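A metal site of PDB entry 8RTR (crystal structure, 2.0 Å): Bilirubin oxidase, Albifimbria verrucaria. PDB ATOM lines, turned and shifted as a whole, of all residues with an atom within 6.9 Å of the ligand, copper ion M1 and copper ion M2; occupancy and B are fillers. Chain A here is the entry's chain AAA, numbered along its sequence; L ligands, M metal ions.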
ATOM      1  N   HIS A  94     -29.195  33.745   3.606  1.00  0.00           N
ATOM      2  CA  HIS A  94     -28.236  32.952   4.407  1.00  0.00           C
ATOM      3  C   HIS A  94     -26.904  32.808   3.680  1.00  0.00           C
ATOM      4  O   HIS A  94     -26.918  32.330   2.533  1.00  0.00           O
ATOM      5  CB  HIS A  94     -28.839  31.591   4.691  1.00  0.00           C
ATOM      6  CG  HIS A  94     -27.893  30.651   5.340  1.00  0.00           C
ATOM      7  ND1 HIS A  94     -27.249  30.971   6.502  1.00  0.00           N
ATOM      8  CD2 HIS A  94     -27.517  29.403   5.015  1.00  0.00           C
ATOM      9  CE1 HIS A  94     -26.492  29.968   6.861  1.00  0.00           C
ATOM     10  NE2 HIS A  94     -26.659  28.990   5.969  1.00  0.00           N
ATOM     11  N   LEU A  95     -25.810  33.176   4.348  1.00  0.00           N
ATOM     12  CA  LEU A  95     -24.419  32.832   3.959  1.00  0.00           C
ATOM     13  C   LEU A  95     -24.061  31.474   4.582  1.00  0.00           C
ATOM     14  O   LEU A  95     -23.722  31.406   5.788  1.00  0.00           O
ATOM     15  CB  LEU A  95     -23.435  33.923   4.437  1.00  0.00           C
ATOM     16  CG  LEU A  95     -21.988  33.748   3.983  1.00  0.00           C
ATOM     17  CD1 LEU A  95     -21.890  33.650   2.485  1.00  0.00           C
ATOM     18  CD2 LEU A  95     -21.117  34.906   4.463  1.00  0.00           C
ATOM     19  N   HIS A  96     -24.196  30.431   3.782  1.00  0.00           N
ATOM     20  CA  HIS A  96     -23.966  29.027   4.159  1.00  0.00           C
ATOM     21  C   HIS A  96     -22.436  28.806   4.245  1.00  0.00           C
ATOM     22  O   HIS A  96     -21.724  28.947   3.239  1.00  0.00           O
ATOM     23  CB  HIS A  96     -24.736  28.150   3.146  1.00  0.00           C
ATOM     24  CG  HIS A  96     -24.770  26.696   3.487  1.00  0.00           C
ATOM     25  ND1 HIS A  96     -25.887  25.923   3.291  1.00  0.00           N
ATOM     26  CD2 HIS A  96     -23.829  25.885   4.032  1.00  0.00           C
ATOM     27  CE1 HIS A  96     -25.627  24.681   3.671  1.00  0.00           C
ATOM     28  NE2 HIS A  96     -24.377  24.624   4.150  1.00  0.00           N
ATOM     29  N   GLY A  97     -21.945  28.496   5.438  1.00  0.00           N
ATOM     30  CA  GLY A  97     -20.520  28.259   5.693  1.00  0.00           C
ATOM     31  C   GLY A  97     -19.944  29.309   6.626  1.00  0.00           C
ATOM     32  O   GLY A  97     -18.758  29.168   6.918  1.00  0.00           O
ATOM     33  N   ASP A 105     -27.938  35.630   9.817  1.00  0.00           N
ATOM     34  CA  ASP A 105     -27.711  34.221   9.421  1.00  0.00           C
ATOM     35  C   ASP A 105     -28.789  33.728   8.463  1.00  0.00           C
ATOM     36  O   ASP A 105     -28.613  32.652   7.899  1.00  0.00           O
ATOM     37  CB  ASP A 105     -27.634  33.271  10.618  1.00  0.00           C
ATOM     38  CG  ASP A 105     -27.012  31.908  10.290  1.00  0.00           C
ATOM     39  OD1 ASP A 105     -25.927  31.889   9.610  1.00  0.00           O
ATOM     40  OD2 ASP A 105     -27.615  30.884  10.714  1.00  0.00           O
ATOM     41  N   GLY A 106     -29.849  34.494   8.250  1.00  0.00           N
ATOM     42  CA  GLY A 106     -30.926  34.071   7.341  1.00  0.00           C
ATOM     43  C   GLY A 106     -31.959  33.205   8.044  1.00  0.00           C
ATOM     44  O   GLY A 106     -32.600  32.372   7.373  1.00  0.00           O
ATOM     45  N   TRP A 132     -21.589  29.780   0.099  1.00  0.00           N
ATOM     46  CA  TRP A 132     -22.571  30.222  -0.904  1.00  0.00           C
ATOM     47  C   TRP A 132     -23.670  30.981  -0.167  1.00  0.00           C
ATOM     48  O   TRP A 132     -23.910  30.650   1.010  1.00  0.00           O
ATOM     49  CB  TRP A 132     -23.044  29.063  -1.793  1.00  0.00           C
ATOM     50  CG  TRP A 132     -23.824  27.974  -1.112  1.00  0.00           C
ATOM     51  CD1 TRP A 132     -23.426  27.182  -0.075  1.00  0.00           C
ATOM     52  CD2 TRP A 132     -25.115  27.480  -1.524  1.00  0.00           C
ATOM     53  NE1 TRP A 132     -24.406  26.267   0.232  1.00  0.00           N
ATOM     54  CE2 TRP A 132     -25.440  26.412  -0.646  1.00  0.00           C
ATOM     55  CE3 TRP A 132     -26.009  27.808  -2.545  1.00  0.00           C
ATOM     56  CZ2 TRP A 132     -26.623  25.687  -0.771  1.00  0.00           C
ATOM     57  CZ3 TRP A 132     -27.188  27.100  -2.656  1.00  0.00           C
ATOM     58  CH2 TRP A 132     -27.501  26.071  -1.771  1.00  0.00           C
ATOM     59  N   HIS A 134     -27.729  32.317  -0.374  1.00  0.00           N
ATOM     60  CA  HIS A 134     -28.996  31.853  -0.995  1.00  0.00           C
ATOM     61  C   HIS A 134     -30.163  32.147  -0.077  1.00  0.00           C
ATOM     62  O   HIS A 134     -29.979  32.415   1.135  1.00  0.00           O
ATOM     63  CB  HIS A 134     -28.952  30.348  -1.343  1.00  0.00           C
ATOM     64  CG  HIS A 134     -28.869  29.442  -0.157  1.00  0.00           C
ATOM     65  ND1 HIS A 134     -29.933  29.201   0.651  1.00  0.00           N
ATOM     66  CD2 HIS A 134     -27.867  28.692   0.338  1.00  0.00           C
ATOM     67  CE1 HIS A 134     -29.616  28.331   1.602  1.00  0.00           C
ATOM     68  NE2 HIS A 134     -28.352  27.993   1.423  1.00  0.00           N
ATOM     69  N   ASP A 135     -31.350  32.018  -0.651  1.00  0.00           N
ATOM     70  CA  ASP A 135     -32.564  32.418   0.061  1.00  0.00           C
ATOM     71  C   ASP A 135     -32.868  31.376   1.121  1.00  0.00           C
ATOM     72  O   ASP A 135     -32.555  30.161   0.882  1.00  0.00           O
ATOM     73  CB  ASP A 135     -33.729  32.630  -0.895  1.00  0.00           C
ATOM     74  CG  ASP A 135     -34.848  33.319  -0.161  1.00  0.00           C
ATOM     75  OD1 ASP A 135     -34.623  34.477   0.320  1.00  0.00           O
ATOM     76  OD2 ASP A 135     -35.888  32.673   0.029  1.00  0.00           O
ATOM     77  N   HIS A 136     -33.472  31.817   2.212  1.00  0.00           N
ATOM     78  CA  HIS A 136     -33.887  30.932   3.328  1.00  0.00           C
ATOM     79  C   HIS A 136     -35.282  31.309   3.833  1.00  0.00           C
ATOM     80  O   HIS A 136     -35.637  30.914   4.956  1.00  0.00           O
ATOM     81  CB  HIS A 136     -32.811  31.036   4.397  1.00  0.00           C
ATOM     82  CG  HIS A 136     -32.542  29.769   5.129  1.00  0.00           C
ATOM     83  ND1 HIS A 136     -33.520  29.103   5.807  1.00  0.00           N
ATOM     84  CD2 HIS A 136     -31.383  29.075   5.326  1.00  0.00           C
ATOM     85  CE1 HIS A 136     -33.009  28.005   6.346  1.00  0.00           C
ATOM     86  NE2 HIS A 136     -31.691  27.981   6.098  1.00  0.00           N
ATOM     87  N   THR A 141     -38.310  28.755   0.261  1.00  0.00           N
ATOM     88  CA  THR A 141     -36.854  28.658  -0.016  1.00  0.00           C
ATOM     89  C   THR A 141     -36.645  27.857  -1.320  1.00  0.00           C
ATOM     90  O   THR A 141     -35.815  28.251  -2.119  1.00  0.00           O
ATOM     91  CB  THR A 141     -36.108  28.011   1.158  1.00  0.00           C
ATOM     92  OG1 THR A 141     -36.274  28.893   2.250  1.00  0.00           O
ATOM     93  CG2 THR A 141     -34.639  27.798   0.847  1.00  0.00           C
ATOM     94  N   ALA A 274     -26.292  21.290  -1.077  1.00  0.00           N
ATOM     95  CA  ALA A 274     -25.601  22.284  -0.228  1.00  0.00           C
ATOM     96  C   ALA A 274     -24.168  21.843   0.099  1.00  0.00           C
ATOM     97  O   ALA A 274     -23.444  22.631   0.686  1.00  0.00           O
ATOM     98  CB  ALA A 274     -26.381  22.567   1.032  1.00  0.00           C
ATOM     99  N   ARG A 276     -20.316  21.395  -0.654  1.00  0.00           N
ATOM    100  CA  ARG A 276     -19.216  21.926  -1.523  1.00  0.00           C
ATOM    101  C   ARG A 276     -18.049  20.949  -1.432  1.00  0.00           C
ATOM    102  O   ARG A 276     -17.633  20.586  -0.299  1.00  0.00           O
ATOM    103  CB  ARG A 276     -18.744  23.330  -1.120  1.00  0.00           C
ATOM    104  CG  ARG A 276     -19.763  24.452  -1.324  1.00  0.00           C
ATOM    105  CD  ARG A 276     -20.764  24.528  -0.183  1.00  0.00           C
ATOM    106  NE  ARG A 276     -20.174  25.005   1.064  1.00  0.00           N
ATOM    107  CZ  ARG A 276     -20.642  24.738   2.278  1.00  0.00           C
ATOM    108  NH1 ARG A 276     -20.032  25.218   3.341  1.00  0.00           N
ATOM    109  NH2 ARG A 276     -21.709  23.969   2.432  1.00  0.00           N
ATOM    110  N   HIS A 401     -28.017  19.728   7.450  1.00  0.00           N
ATOM    111  CA  HIS A 401     -27.188  20.935   7.613  1.00  0.00           C
ATOM    112  C   HIS A 401     -27.393  21.474   9.018  1.00  0.00           C
ATOM    113  O   HIS A 401     -28.531  21.511   9.471  1.00  0.00           O
ATOM    114  CB  HIS A 401     -27.564  21.951   6.545  1.00  0.00           C
ATOM    115  CG  HIS A 401     -26.830  23.228   6.696  1.00  0.00           C
ATOM    116  ND1 HIS A 401     -25.466  23.270   6.962  1.00  0.00           N
ATOM    117  CD2 HIS A 401     -27.260  24.509   6.608  1.00  0.00           C
ATOM    118  CE1 HIS A 401     -25.098  24.521   7.043  1.00  0.00           C
ATOM    119  NE2 HIS A 401     -26.194  25.303   6.853  1.00  0.00           N
ATOM    120  N   ILE A 402     -26.315  21.891   9.660  1.00  0.00           N
ATOM    121  CA  ILE A 402     -26.390  22.572  10.965  1.00  0.00           C
ATOM    122  C   ILE A 402     -25.722  23.945  10.785  1.00  0.00           C
ATOM    123  O   ILE A 402     -24.498  24.010  10.445  1.00  0.00           O
ATOM    124  CB  ILE A 402     -25.721  21.720  12.061  1.00  0.00           C
ATOM    125  CG1 ILE A 402     -26.252  20.288  12.120  1.00  0.00           C
ATOM    126  CG2 ILE A 402     -25.831  22.437  13.395  1.00  0.00           C
ATOM    127  CD1 ILE A 402     -25.454  19.366  13.019  1.00  0.00           C
ATOM    128  N   HIS A 403     -26.472  25.001  11.084  1.00  0.00           N
ATOM    129  CA  HIS A 403     -25.978  26.399  11.047  1.00  0.00           C
ATOM    130  C   HIS A 403     -24.926  26.600  12.147  1.00  0.00           C
ATOM    131  O   HIS A 403     -24.799  25.756  13.032  1.00  0.00           O
ATOM    132  CB  HIS A 403     -27.156  27.395  11.175  1.00  0.00           C
ATOM    133  CG  HIS A 403     -27.994  27.484   9.942  1.00  0.00           C
ATOM    134  ND1 HIS A 403     -28.264  28.669   9.337  1.00  0.00           N
ATOM    135  CD2 HIS A 403     -28.599  26.523   9.197  1.00  0.00           C
ATOM    136  CE1 HIS A 403     -29.047  28.462   8.290  1.00  0.00           C
ATOM    137  NE2 HIS A 403     -29.259  27.129   8.173  1.00  0.00           N
ATOM    138  N   VAL A 431     -22.774  20.058   5.983  1.00  0.00           N
ATOM    139  CA  VAL A 431     -23.861  19.228   5.427  1.00  0.00           C
ATOM    140  C   VAL A 431     -23.404  17.757   5.448  1.00  0.00           C
ATOM    141  O   VAL A 431     -22.226  17.501   5.120  1.00  0.00           O
ATOM    142  CB  VAL A 431     -24.191  19.681   4.001  1.00  0.00           C
ATOM    143  CG1 VAL A 431     -25.424  18.974   3.436  1.00  0.00           C
ATOM    144  CG2 VAL A 431     -24.400  21.191   3.943  1.00  0.00           C
ATOM    145  N   MET A 454     -30.751  27.513  13.085  1.00  0.00           N
ATOM    146  CA  MET A 454     -31.503  26.448  12.412  1.00  0.00           C
ATOM    147  C   MET A 454     -30.597  25.237  12.164  1.00  0.00           C
ATOM    148  O   MET A 454     -29.345  25.372  12.078  1.00  0.00           O
ATOM    149  CB  MET A 454     -32.067  26.959  11.087  1.00  0.00           C
ATOM    150  CG  MET A 454     -33.095  28.063  11.293  1.00  0.00           C
ATOM    151  SD  MET A 454     -33.712  28.817   9.789  1.00  0.00           S
ATOM    152  CE  MET A 454     -32.210  29.467   9.070  1.00  0.00           C
ATOM    153  N   PHE A 455     -31.230  24.079  12.052  1.00  0.00           N
ATOM    154  CA  PHE A 455     -30.665  22.853  11.434  1.00  0.00           C
ATOM    155  C   PHE A 455     -31.831  22.140  10.757  1.00  0.00           C
ATOM    156  O   PHE A 455     -32.998  22.311  11.177  1.00  0.00           O
ATOM    157  CB  PHE A 455     -29.932  21.976  12.456  1.00  0.00           C
ATOM    158  CG  PHE A 455     -30.790  21.210  13.430  1.00  0.00           C
ATOM    159  CD1 PHE A 455     -31.343  21.852  14.529  1.00  0.00           C
ATOM    160  CD2 PHE A 455     -31.020  19.846  13.278  1.00  0.00           C
ATOM    161  CE1 PHE A 455     -32.113  21.138  15.443  1.00  0.00           C
ATOM    162  CE2 PHE A 455     -31.780  19.141  14.192  1.00  0.00           C
ATOM    163  CZ  PHE A 455     -32.315  19.796  15.279  1.00  0.00           C
ATOM    164  N   HIS A 456     -31.539  21.443   9.683  1.00  0.00           N
ATOM    165  CA  HIS A 456     -32.606  20.989   8.775  1.00  0.00           C
ATOM    166  C   HIS A 456     -32.009  20.126   7.682  1.00  0.00           C
ATOM    167  O   HIS A 456     -30.797  20.212   7.424  1.00  0.00           O
ATOM    168  CB  HIS A 456     -33.331  22.199   8.155  1.00  0.00           C
ATOM    169  CG  HIS A 456     -32.419  23.120   7.421  1.00  0.00           C
ATOM    170  ND1 HIS A 456     -32.238  23.056   6.060  1.00  0.00           N
ATOM    171  CD2 HIS A 456     -31.649  24.139   7.856  1.00  0.00           C
ATOM    172  CE1 HIS A 456     -31.414  24.011   5.704  1.00  0.00           C
ATOM    173  NE2 HIS A 456     -31.037  24.674   6.784  1.00  0.00           N
ATOM    174  N   CYS A 457     -32.909  19.473   6.959  1.00  0.00           N
ATOM    175  CA  CYS A 457     -32.588  18.862   5.657  1.00  0.00           C
ATOM    176  C   CYS A 457     -32.477  19.982   4.609  1.00  0.00           C
ATOM    177  O   CYS A 457     -33.262  20.957   4.662  1.00  0.00           O
ATOM    178  CB  CYS A 457     -33.614  17.792   5.353  1.00  0.00           C
ATOM    179  SG  CYS A 457     -33.415  17.099   3.698  1.00  0.00           S
ATOM    180  N   HIS A 458     -31.529  19.844   3.687  1.00  0.00           N
ATOM    181  CA  HIS A 458     -31.268  20.798   2.572  1.00  0.00           C
ATOM    182  C   HIS A 458     -31.846  20.310   1.245  1.00  0.00           C
ATOM    183  O   HIS A 458     -31.629  20.980   0.246  1.00  0.00           O
ATOM    184  CB  HIS A 458     -29.771  21.056   2.441  1.00  0.00           C
ATOM    185  CG  HIS A 458     -29.486  22.483   2.120  1.00  0.00           C
ATOM    186  ND1 HIS A 458     -29.754  23.010   0.879  1.00  0.00           N
ATOM    187  CD2 HIS A 458     -29.002  23.489   2.872  1.00  0.00           C
ATOM    188  CE1 HIS A 458     -29.434  24.292   0.883  1.00  0.00           C
ATOM    189  NE2 HIS A 458     -28.934  24.599   2.086  1.00  0.00           N
ATOM    190  N   LEU A 460     -34.793  21.152  -0.438  1.00  0.00           N
ATOM    191  CA  LEU A 460     -35.483  22.412  -0.142  1.00  0.00           C
ATOM    192  C   LEU A 460     -37.001  22.157  -0.100  1.00  0.00           C
ATOM    193  O   LEU A 460     -37.706  22.863   0.606  1.00  0.00           O
ATOM    194  CB  LEU A 460     -35.074  23.435  -1.189  1.00  0.00           C
ATOM    195  CG  LEU A 460     -33.578  23.794  -1.230  1.00  0.00           C
ATOM    196  CD1 LEU A 460     -33.352  24.915  -2.220  1.00  0.00           C
ATOM    197  CD2 LEU A 460     -33.053  24.204   0.131  1.00  0.00           C
ATOM    198  N   GLU A 463     -37.369  20.815   3.437  1.00  0.00           N
ATOM    199  CA  GLU A 463     -37.083  21.984   4.320  1.00  0.00           C
ATOM    200  C   GLU A 463     -38.332  22.881   4.450  1.00  0.00           C
ATOM    201  O   GLU A 463     -38.682  23.269   5.574  1.00  0.00           O
ATOM    202  CB  GLU A 463     -35.918  22.802   3.744  1.00  0.00           C
ATOM    203  CG  GLU A 463     -35.461  23.936   4.610  1.00  0.00           C
ATOM    204  CD  GLU A 463     -34.319  24.727   4.021  1.00  0.00           C
ATOM    205  OE1 GLU A 463     -33.455  24.090   3.296  1.00  0.00           O
ATOM    206  OE2 GLU A 463     -34.262  25.963   4.307  1.00  0.00           O
ATOM    207  N   MET A 468     -37.255  21.136   9.444  1.00  0.00           N
ATOM    208  CA  MET A 468     -36.337  22.141   9.990  1.00  0.00           C
ATOM    209  C   MET A 468     -36.682  22.376  11.443  1.00  0.00           C
ATOM    210  O   MET A 468     -37.850  22.200  11.805  1.00  0.00           O
ATOM    211  CB  MET A 468     -36.466  23.436   9.201  1.00  0.00           C
ATOM    212  CG  MET A 468     -35.531  24.549   9.644  1.00  0.00           C
ATOM    213  SD  MET A 468     -35.276  25.587   8.192  1.00  0.00           S
ATOM    214  CE  MET A 468     -36.890  26.387   8.116  1.00  0.00           C
HETATM  215  O1  LIG L   1     -28.761  26.449   4.865  1.00  0.00           O
HETATM  216  O2  LIG L   1     -29.566  26.740   4.142  1.00  0.00           O
HETATM  217 CU    CU M   1     -30.366  26.677   6.597  1.00  0.00          CU
HETATM  218 CU    CU M   2     -27.647  26.417   2.566  1.00  0.00          CU
HETATM  219 CU    CU M   3     -26.420  27.157   6.370  1.00  0.00          CU
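ND1 of His 96 binds copper ion M2 (2.0 Å). NE2 of His 134 binds copper ion M2. Copper ion M2 is bound by NE2 of His 458, 2.3 Å away. O2 of the ligand binds copper ion M2 (2.5 Å).
His 401 touches copper ion M1. Of the 25 residues printed, 4 come within 4 Å of copper ion M1.
CD2 of His 94 touches copper ion M2 (3.9 Å). Trp 132 touches copper ion M2. Along chain A the residues within 4 Å of copper ion M2 span positions 94 to 458. The nearest printed residue that does not touch copper ion M2 is Ala 274 (4.3 Å).
The side-chain carboxylate (OE1) of Glu 463 lies close to a ring nitrogen (ND1) of His 456, 3.2 Å away. The backbone carbonyl oxygen (O) of Trp 132 sits at hydrogen-bond distance from the backbone NH (N) of His 96, at 2.8 Å. The backbone carbonyl oxygen (O) of His 136 lies close to the side-chain hydroxyl (OG1) of Thr 141 (3.4 Å). A ring nitrogen (NE2) of His 96 sits at hydrogen-bond distance from the guanidinium group (NH2) of Arg 276, 3.2 Å away. The backbone NH (N) of His 403 lies within hydrogen-bond range of the backbone carbonyl oxygen (O) of Met 454, at 3.1 Å. The backbone carbonyl oxygen of His 134 lies within hydrogen-bond range of the backbone NH of His 94, 2.9 Å away. O of His 456 lies within hydrogen-bond range of N of His 401 (2.8 Å). A ring nitrogen (NE2) of His 96 sits close to a ring nitrogen (ND1) of His 401, at 3.3 Å.
A ring nitrogen (NE2) of His 94 sits close to an oxygen (O1) of the ligand, 3.5 Å away. An oxygen (O1) of the ligand lies close to a ring nitrogen (NE2) of His 401, 3.4 Å away. Hydrophobic or aromatic side chains within 4 Å of the ligand: His 94, His 96, His 134, His 136, His 401, His 403, His 456 and His 458. Along chain A the residues within 4 Å of the ligand span positions 94 to 458.
Copper ion M1 is bound by NE2 of His 136. NE2 of His 403 is bound to copper ion M1 (2.0 Å). Copper ion M1 is bound by NE2 of His 456, at 2.1 Å. Copper ion M1 is bound by an oxygen (O1) of the ligand, at 2.4 Å. Copper ion M1 has four donor atoms within binding distance.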
